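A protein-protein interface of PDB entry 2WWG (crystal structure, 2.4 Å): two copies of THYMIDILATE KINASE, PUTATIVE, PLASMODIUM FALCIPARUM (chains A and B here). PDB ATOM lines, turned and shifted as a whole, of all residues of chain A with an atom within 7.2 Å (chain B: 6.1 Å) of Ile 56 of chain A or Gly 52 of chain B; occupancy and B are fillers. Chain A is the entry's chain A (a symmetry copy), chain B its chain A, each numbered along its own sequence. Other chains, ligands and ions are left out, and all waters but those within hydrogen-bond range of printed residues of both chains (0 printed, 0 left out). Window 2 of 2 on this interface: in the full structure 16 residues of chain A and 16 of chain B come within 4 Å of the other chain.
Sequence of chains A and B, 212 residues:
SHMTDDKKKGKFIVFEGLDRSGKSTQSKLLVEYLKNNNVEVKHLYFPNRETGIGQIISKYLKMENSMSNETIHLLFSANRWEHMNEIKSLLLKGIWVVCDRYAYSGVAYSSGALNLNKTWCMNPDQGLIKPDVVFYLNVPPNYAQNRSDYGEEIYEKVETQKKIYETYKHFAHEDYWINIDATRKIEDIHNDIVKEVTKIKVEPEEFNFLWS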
ATOM      1  N   ARG A  49       2.704  -3.564  15.253  1.00  0.00           N
ATOM      2  CA  ARG A  49       2.797  -4.973  14.873  1.00  0.00           C
ATOM      3  C   ARG A  49       3.978  -5.316  13.963  1.00  0.00           C
ATOM      4  O   ARG A  49       4.129  -6.472  13.604  1.00  0.00           O
ATOM      5  CB  ARG A  49       1.494  -5.477  14.276  1.00  0.00           C
ATOM      6  CG  ARG A  49       0.277  -5.229  15.197  1.00  0.00           C
ATOM      7  CD  ARG A  49      -0.983  -5.431  14.323  1.00  0.00           C
ATOM      8  NE  ARG A  49      -2.286  -5.189  14.946  1.00  0.00           N
ATOM      9  CZ  ARG A  49      -3.263  -6.096  14.948  1.00  0.00           C
ATOM     10  NH1 ARG A  49      -3.058  -7.314  14.420  1.00  0.00           N
ATOM     11  NH2 ARG A  49      -4.437  -5.812  15.466  1.00  0.00           N
ATOM     12  N   THR A  51       7.377  -4.788  14.577  1.00  0.00           N
ATOM     13  CA  THR A  51       8.644  -5.215  15.234  1.00  0.00           C
ATOM     14  C   THR A  51       8.583  -6.696  15.556  1.00  0.00           C
ATOM     15  O   THR A  51       7.530  -7.330  15.404  1.00  0.00           O
ATOM     16  CB  THR A  51       8.838  -4.489  16.561  1.00  0.00           C
ATOM     17  OG1 THR A  51       7.819  -4.926  17.462  1.00  0.00           O
ATOM     18  CG2 THR A  51       8.746  -2.912  16.380  1.00  0.00           C
ATOM     19  N   GLY A  52       9.694  -7.256  16.039  1.00  0.00           N
ATOM     20  CA  GLY A  52       9.693  -8.676  16.447  1.00  0.00           C
ATOM     21  C   GLY A  52       8.643  -8.908  17.508  1.00  0.00           C
ATOM     22  O   GLY A  52       7.887  -9.891  17.434  1.00  0.00           O
ATOM     23  N   ILE A  53       8.556  -7.993  18.483  1.00  0.00           N
ATOM     24  CA  ILE A  53       7.573  -8.165  19.565  1.00  0.00           C
ATOM     25  C   ILE A  53       6.157  -7.963  18.990  1.00  0.00           C
ATOM     26  O   ILE A  53       5.239  -8.766  19.263  1.00  0.00           O
ATOM     27  CB  ILE A  53       7.835  -7.188  20.716  1.00  0.00           C
ATOM     28  CG1 ILE A  53       9.150  -7.562  21.367  1.00  0.00           C
ATOM     29  CG2 ILE A  53       6.684  -7.200  21.697  1.00  0.00           C
ATOM     30  CD1 ILE A  53       9.788  -6.422  22.090  1.00  0.00           C
ATOM     31  N   GLY A  54       6.018  -6.926  18.150  1.00  0.00           N
ATOM     32  CA  GLY A  54       4.774  -6.687  17.431  1.00  0.00           C
ATOM     33  C   GLY A  54       4.204  -7.866  16.663  1.00  0.00           C
ATOM     34  O   GLY A  54       2.974  -8.115  16.707  1.00  0.00           O
ATOM     35  N   GLN A  55       5.082  -8.627  16.013  1.00  0.00           N
ATOM     36  CA  GLN A  55       4.653  -9.794  15.227  1.00  0.00           C
ATOM     37  C   GLN A  55       3.971 -10.866  16.109  1.00  0.00           C
ATOM     38  O   GLN A  55       2.888 -11.406  15.746  1.00  0.00           O
ATOM     39  CB  GLN A  55       5.829 -10.314  14.392  1.00  0.00           C
ATOM     40  CG  GLN A  55       6.260  -9.271  13.270  1.00  0.00           C
ATOM     41  CD  GLN A  55       7.497  -9.673  12.435  1.00  0.00           C
ATOM     42  OE1 GLN A  55       8.428  -8.854  12.168  1.00  0.00           O
ATOM     43  NE2 GLN A  55       7.516 -10.939  12.021  1.00  0.00           N
ATOM     44  N   ILE A  56       4.524 -11.093  17.300  1.00  0.00           N
ATOM     45  CA  ILE A  56       3.933 -12.045  18.209  1.00  0.00           C
ATOM     46  C   ILE A  56       2.639 -11.490  18.751  1.00  0.00           C
ATOM     47  O   ILE A  56       1.627 -12.208  18.804  1.00  0.00           O
ATOM     48  CB  ILE A  56       4.879 -12.422  19.416  1.00  0.00           C
ATOM     49  CG1 ILE A  56       6.150 -13.101  18.913  1.00  0.00           C
ATOM     50  CG2 ILE A  56       4.140 -13.245  20.472  1.00  0.00           C
ATOM     51  CD1 ILE A  56       7.377 -12.696  19.714  1.00  0.00           C
ATOM     52  N   ILE A  57       2.648 -10.217  19.149  1.00  0.00           N
ATOM     53  CA  ILE A  57       1.371  -9.594  19.526  1.00  0.00           C
ATOM     54  C   ILE A  57       0.326  -9.819  18.414  1.00  0.00           C
ATOM     55  O   ILE A  57      -0.821 -10.266  18.641  1.00  0.00           O
ATOM     56  CB  ILE A  57       1.526  -8.082  19.884  1.00  0.00           C
ATOM     57  CG1 ILE A  57       2.299  -7.937  21.202  1.00  0.00           C
ATOM     58  CG2 ILE A  57       0.175  -7.482  20.079  1.00  0.00           C
ATOM     59  CD1 ILE A  57       2.793  -6.575  21.477  1.00  0.00           C
ATOM     60  N   SER A  58       0.739  -9.590  17.190  1.00  0.00           N
ATOM     61  CA  SER A  58      -0.214  -9.721  16.104  1.00  0.00           C
ATOM     62  C   SER A  58      -0.736 -11.162  15.982  1.00  0.00           C
ATOM     63  O   SER A  58      -1.963 -11.376  15.814  1.00  0.00           O
ATOM     64  CB  SER A  58       0.422  -9.254  14.801  1.00  0.00           C
ATOM     65  OG  SER A  58      -0.551  -9.235  13.782  1.00  0.00           O
ATOM     66  N   LYS A  59       0.154 -12.159  16.088  1.00  0.00           N
ATOM     67  CA  LYS A  59      -0.328 -13.533  16.020  1.00  0.00           C
ATOM     68  C   LYS A  59      -1.292 -13.780  17.181  1.00  0.00           C
ATOM     69  O   LYS A  59      -2.263 -14.509  17.060  1.00  0.00           O
ATOM     70  CB  LYS A  59       0.856 -14.536  15.983  1.00  0.00           C
ATOM     71  CG  LYS A  59       1.753 -14.494  14.656  1.00  0.00           C
ATOM     72  CD  LYS A  59       3.067 -15.271  14.846  1.00  0.00           C
ATOM     73  CE  LYS A  59       4.290 -14.740  13.968  1.00  0.00           C
ATOM     74  NZ  LYS A  59       5.626 -14.388  14.726  1.00  0.00           N
ATOM     75  N   TYR A  60      -1.076 -13.118  18.303  1.00  0.00           N
ATOM     76  CA  TYR A  60      -1.924 -13.360  19.425  1.00  0.00           C
ATOM     77  C   TYR A  60      -3.348 -12.826  19.164  1.00  0.00           C
ATOM     78  O   TYR A  60      -4.336 -13.514  19.462  1.00  0.00           O
ATOM     79  CB  TYR A  60      -1.323 -12.800  20.690  1.00  0.00           C
ATOM     80  CG  TYR A  60      -2.326 -12.669  21.819  1.00  0.00           C
ATOM     81  CD1 TYR A  60      -2.526 -13.690  22.737  1.00  0.00           C
ATOM     82  CD2 TYR A  60      -3.066 -11.470  21.978  1.00  0.00           C
ATOM     83  CE1 TYR A  60      -3.453 -13.557  23.784  1.00  0.00           C
ATOM     84  CE2 TYR A  60      -3.983 -11.312  22.994  1.00  0.00           C
ATOM     85  CZ  TYR A  60      -4.208 -12.359  23.869  1.00  0.00           C
ATOM     86  OH  TYR A  60      -5.104 -12.138  24.870  1.00  0.00           O
ATOM     87  N   LEU A  61      -3.438 -11.621  18.597  1.00  0.00           N
ATOM     88  CA  LEU A  61      -4.731 -10.969  18.352  1.00  0.00           C
ATOM     89  C   LEU A  61      -5.531 -11.685  17.279  1.00  0.00           C
ATOM     90  O   LEU A  61      -6.770 -11.684  17.304  1.00  0.00           O
ATOM     91  CB  LEU A  61      -4.517  -9.505  17.960  1.00  0.00           C
ATOM     92  CG  LEU A  61      -3.950  -8.640  19.105  1.00  0.00           C
ATOM     93  CD1 LEU A  61      -3.470  -7.304  18.562  1.00  0.00           C
ATOM     94  CD2 LEU A  61      -4.938  -8.470  20.296  1.00  0.00           C
ATOM     95  N   LYS A  62      -4.821 -12.339  16.358  1.00  0.00           N
ATOM     96  CA  LYS A  62      -5.526 -13.116  15.315  1.00  0.00           C
ATOM     97  C   LYS A  62      -5.921 -14.513  15.720  1.00  0.00           C
ATOM     98  O   LYS A  62      -6.437 -15.269  14.905  1.00  0.00           O
ATOM     99  CB  LYS A  62      -4.724 -13.190  14.044  1.00  0.00           C
ATOM    100  CG  LYS A  62      -4.621 -11.844  13.378  1.00  0.00           C
ATOM    101  CD  LYS A  62      -3.613 -11.975  12.265  1.00  0.00           C
ATOM    102  CE  LYS A  62      -3.280 -10.660  11.683  1.00  0.00           C
ATOM    103  NZ  LYS A  62      -1.914 -10.862  11.148  1.00  0.00           N
ATOM    104  N   ASN A  65      -1.785 -17.841  17.710  1.00  0.00           N
ATOM    105  CA  ASN A  65      -1.072 -18.496  18.823  1.00  0.00           C
ATOM    106  C   ASN A  65      -1.898 -18.231  20.068  1.00  0.00           C
ATOM    107  O   ASN A  65      -2.887 -17.471  20.029  1.00  0.00           O
ATOM    108  CB  ASN A  65       0.374 -17.968  19.049  1.00  0.00           C
ATOM    109  CG  ASN A  65       0.415 -16.476  19.449  1.00  0.00           C
ATOM    110  OD1 ASN A  65      -0.477 -15.990  20.166  1.00  0.00           O
ATOM    111  ND2 ASN A  65       1.453 -15.736  18.975  1.00  0.00           N
ATOM    112  N   MET A  67      -1.060 -17.658  24.567  1.00  0.00           N
ATOM    113  CA  MET A  67      -0.005 -17.408  25.579  1.00  0.00           C
ATOM    114  C   MET A  67      -0.710 -17.076  26.900  1.00  0.00           C
ATOM    115  O   MET A  67      -1.852 -16.663  26.880  1.00  0.00           O
ATOM    116  CB  MET A  67       0.845 -16.178  25.207  1.00  0.00           C
ATOM    117  CG  MET A  67       1.020 -15.960  23.709  1.00  0.00           C
ATOM    118  SD  MET A  67       1.855 -14.418  23.234  1.00  0.00           S
ATOM    119  CE  MET A  67       2.442 -14.029  24.769  1.00  0.00           C
ATOM    120  N   THR A  71       2.119 -13.034  30.030  1.00  0.00           N
ATOM    121  CA  THR A  71       3.085 -12.918  28.959  1.00  0.00           C
ATOM    122  C   THR A  71       2.634 -11.919  27.895  1.00  0.00           C
ATOM    123  O   THR A  71       3.405 -11.107  27.441  1.00  0.00           O
ATOM    124  CB  THR A  71       3.268 -14.336  28.282  1.00  0.00           C
ATOM    125  OG1 THR A  71       3.658 -15.276  29.303  1.00  0.00           O
ATOM    126  CG2 THR A  71       4.303 -14.297  27.149  1.00  0.00           C
ATOM    127  N   ILE A  72       1.385 -12.022  27.455  1.00  0.00           N
ATOM    128  CA  ILE A  72       0.904 -11.105  26.454  1.00  0.00           C
ATOM    129  C   ILE A  72       0.886  -9.665  27.014  1.00  0.00           C
ATOM    130  O   ILE A  72       1.389  -8.770  26.367  1.00  0.00           O
ATOM    131  CB  ILE A  72      -0.457 -11.556  25.823  1.00  0.00           C
ATOM    132  CG1 ILE A  72      -0.719 -10.749  24.565  1.00  0.00           C
ATOM    133  CG2 ILE A  72      -1.571 -11.403  26.754  1.00  0.00           C
ATOM    134  CD1 ILE A  72       0.334 -10.912  23.450  1.00  0.00           C
ATOM    135  N   LEU A  75       4.362  -8.371  26.844  1.00  0.00           N
ATOM    136  CA  LEU A  75       4.742  -8.081  25.485  1.00  0.00           C
ATOM    137  C   LEU A  75       4.161  -6.733  25.034  1.00  0.00           C
ATOM    138  O   LEU A  75       4.823  -6.006  24.332  1.00  0.00           O
ATOM    139  CB  LEU A  75       4.257  -9.166  24.565  1.00  0.00           C
ATOM    140  CG  LEU A  75       5.017 -10.484  24.675  1.00  0.00           C
ATOM    141  CD1 LEU A  75       4.754 -11.304  23.474  1.00  0.00           C
ATOM    142  CD2 LEU A  75       6.494 -10.226  24.850  1.00  0.00           C
ATOM    143  N   GLU B  50      14.160 -20.908  22.776  1.00  0.00           N
ATOM    144  CA  GLU B  50      13.528 -21.608  21.695  1.00  0.00           C
ATOM    145  C   GLU B  50      12.117 -21.078  21.379  1.00  0.00           C
ATOM    146  O   GLU B  50      11.552 -21.452  20.350  1.00  0.00           O
ATOM    147  CB  GLU B  50      13.433 -23.137  21.996  1.00  0.00           C
ATOM    148  CG  GLU B  50      14.782 -23.912  22.204  1.00  0.00           C
ATOM    149  CD  GLU B  50      15.888 -23.423  21.286  1.00  0.00           C
ATOM    150  OE1 GLU B  50      15.756 -23.655  20.085  1.00  0.00           O
ATOM    151  OE2 GLU B  50      16.884 -22.795  21.731  1.00  0.00           O
ATOM    152  N   THR B  51      11.513 -20.264  22.247  1.00  0.00           N
ATOM    153  CA  THR B  51      10.175 -19.676  21.952  1.00  0.00           C
ATOM    154  C   THR B  51      10.337 -18.427  21.105  1.00  0.00           C
ATOM    155  O   THR B  51      11.463 -17.960  20.882  1.00  0.00           O
ATOM    156  CB  THR B  51       9.479 -19.241  23.238  1.00  0.00           C
ATOM    157  OG1 THR B  51      10.217 -18.155  23.798  1.00  0.00           O
ATOM    158  CG2 THR B  51       9.404 -20.431  24.289  1.00  0.00           C
ATOM    159  N   GLY B  52       9.220 -17.853  20.656  1.00  0.00           N
ATOM    160  CA  GLY B  52       9.291 -16.594  19.886  1.00  0.00           C
ATOM    161  C   GLY B  52       9.978 -15.527  20.704  1.00  0.00           C
ATOM    162  O   GLY B  52      10.849 -14.806  20.187  1.00  0.00           O
ATOM    163  N   ILE B  53       9.630 -15.435  21.995  1.00  0.00           N
ATOM    164  CA  ILE B  53      10.242 -14.403  22.849  1.00  0.00           C
ATOM    165  C   ILE B  53      11.722 -14.759  23.079  1.00  0.00           C
ATOM    166  O   ILE B  53      12.612 -13.889  22.957  1.00  0.00           O
ATOM    167  CB  ILE B  53       9.501 -14.276  24.184  1.00  0.00           C
ATOM    168  CG1 ILE B  53       8.114 -13.735  23.909  1.00  0.00           C
ATOM    169  CG2 ILE B  53      10.279 -13.402  25.143  1.00  0.00           C
ATOM    170  CD1 ILE B  53       7.131 -14.078  24.980  1.00  0.00           C
ATOM    171  N   GLY B  54      11.972 -16.049  23.348  1.00  0.00           N
ATOM    172  CA  GLY B  54      13.333 -16.558  23.461  1.00  0.00           C
ATOM    173  C   GLY B  54      14.271 -16.229  22.314  1.00  0.00           C
ATOM    174  O   GLY B  54      15.447 -15.858  22.546  1.00  0.00           O
ATOM    175  N   GLN B  55      13.753 -16.301  21.089  1.00  0.00           N
ATOM    176  CA  GLN B  55      14.563 -16.013  19.896  1.00  0.00           C
ATOM    177  C   GLN B  55      15.079 -14.555  19.883  1.00  0.00           C
ATOM    178  O   GLN B  55      16.283 -14.299  19.607  1.00  0.00           O
ATOM    179  CB  GLN B  55      13.790 -16.423  18.637  1.00  0.00           C
ATOM    180  CG  GLN B  55      13.590 -18.000  18.558  1.00  0.00           C
ATOM    181  CD  GLN B  55      12.744 -18.499  17.364  1.00  0.00           C
ATOM    182  OE1 GLN B  55      11.837 -19.377  17.498  1.00  0.00           O
ATOM    183  NE2 GLN B  55      13.029 -17.938  16.190  1.00  0.00           N
ATOM    184  N   ILE B  56      14.218 -13.620  20.286  1.00  0.00           N
ATOM    185  CA  ILE B  56      14.622 -12.236  20.349  1.00  0.00           C
ATOM    186  C   ILE B  56      15.593 -12.044  21.488  1.00  0.00           C
ATOM    187  O   ILE B  56      16.627 -11.378  21.320  1.00  0.00           O
ATOM    188  CB  ILE B  56      13.409 -11.242  20.532  1.00  0.00           C
ATOM    189  CG1 ILE B  56      12.465 -11.317  19.336  1.00  0.00           C
ATOM    190  CG2 ILE B  56      13.888  -9.819  20.826  1.00  0.00           C
ATOM    191  CD1 ILE B  56      11.006 -11.187  19.741  1.00  0.00           C
ATOM    192  N   ILE B  57      15.284 -12.624  22.649  1.00  0.00           N
ATOM    193  CA  ILE B  57      16.281 -12.600  23.729  1.00  0.00           C
ATOM    194  C   ILE B  57      17.641 -13.103  23.203  1.00  0.00           C
ATOM    195  O   ILE B  57      18.710 -12.477  23.381  1.00  0.00           O
ATOM    196  CB  ILE B  57      15.814 -13.393  24.992  1.00  0.00           C
ATOM    197  CG1 ILE B  57      14.657 -12.650  25.672  1.00  0.00           C
ATOM    198  CG2 ILE B  57      16.941 -13.474  25.965  1.00  0.00           C
ATOM    199  CD1 ILE B  57      13.918 -13.447  26.669  1.00  0.00           C
ATOM    200  N   LYS B  59      18.852 -13.162  20.130  1.00  0.00           N
ATOM    201  CA  LYS B  59      19.516 -12.209  19.249  1.00  0.00           C
ATOM    202  C   LYS B  59      20.096 -11.072  20.091  1.00  0.00           C
ATOM    203  O   LYS B  59      21.147 -10.529  19.795  1.00  0.00           O
ATOM    204  CB  LYS B  59      18.554 -11.717  18.134  1.00  0.00           C
ATOM    205  CG  LYS B  59      18.118 -12.826  17.062  1.00  0.00           C
ATOM    206  CD  LYS B  59      16.931 -12.342  16.211  1.00  0.00           C
ATOM    207  CE  LYS B  59      15.982 -13.504  15.667  1.00  0.00           C
ATOM    208  NZ  LYS B  59      14.441 -13.383  15.976  1.00  0.00           N
ATOM    209  N   GLU B  82       6.022 -17.503  30.479  1.00  0.00           N
ATOM    210  CA  GLU B  82       5.526 -18.524  29.580  1.00  0.00           C
ATOM    211  C   GLU B  82       5.813 -19.979  30.065  1.00  0.00           C
ATOM    212  O   GLU B  82       5.407 -20.940  29.411  1.00  0.00           O
ATOM    213  CB  GLU B  82       5.917 -18.279  28.094  1.00  0.00           C
ATOM    214  CG  GLU B  82       7.351 -17.934  27.766  1.00  0.00           C
ATOM    215  CD  GLU B  82       7.694 -17.737  26.229  1.00  0.00           C
ATOM    216  OE1 GLU B  82       6.825 -17.831  25.342  1.00  0.00           O
ATOM    217  OE2 GLU B  82       8.903 -17.501  25.919  1.00  0.00           O
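The backbone NH of Glu 82 of chain B sits at hydrogen-bond distance from the side-chain hydroxyl of Thr 71 of chain A, at 3.5 Å.
OG1 of Thr 51 of chain B lies close to N of Ile 53 of chain B, at 3.3 Å. The side-chain carboxylate of Glu 82 of chain B lies within hydrogen-bond range of the side-chain hydroxyl of Thr 51 of chain B, at 2.6 Å.
Gly 52 of chain A touches Ile 56 of chain B. Ile 56 of chain A touches Gly 52 of chain B (CD1 to C, 3.97 Å). CD1 of Ile 56 of chain B touches CD1 of Ile 56 of chain A, at 3.9 Å. Ile 53 of chain B touches Thr 71 of chain A (CD1 to CG2, 3.6 Å). CD1 of Ile 53 of chain B touches CD2 of Leu 75 of chain A, 3.9 Å away.
Of chain B, only Gly 52 (3.97 Å) and Ile 56 (3.9 Å) come within 4 Å of Ile 56 of chain A. Printed residues of chain B within 4 Å of Thr 71 of chain A: Ile 53 (3.6 Å) and Glu 82 (3.5 Å). Gly 52 of chain B touches just one residue of chain A: Ile 56. Printed residues of chain A within 4 Å of Glu 82 of chain B: Thr 71.
Hydrophobic or aromatic side chains of chain A that line the printed part of chain B: Ile 56 and Leu 75. Of the 10 printed residues of chain B, 4 touch a printed residue of chain A. Printed residues of chain B that touch a printed residue of chain A: Gly 52, Ile 53, Ile 56 and Glu 82. Among the printed residues, 6 pairs touch across the chains. Among the printed residues, no Asp or Glu carboxylate lies within 4 Å of a Lys or Arg side-chain nitrogen of the other chain.
Gly 52 of chain A touches Ile 56 of chain B, and with the chains exchanged Ile 56 of chain A touches Gly 52 of chain B. Ile 56 of chain B touches its own counterpart, Ile 56 of chain A. Positions printed for both chains: 51, 52, 53, 54, 55, 56, 57 and 59. Of the 6 pairs that touch across the chains among the printed residues, 3 have their exchanged pair printed and touching as well.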
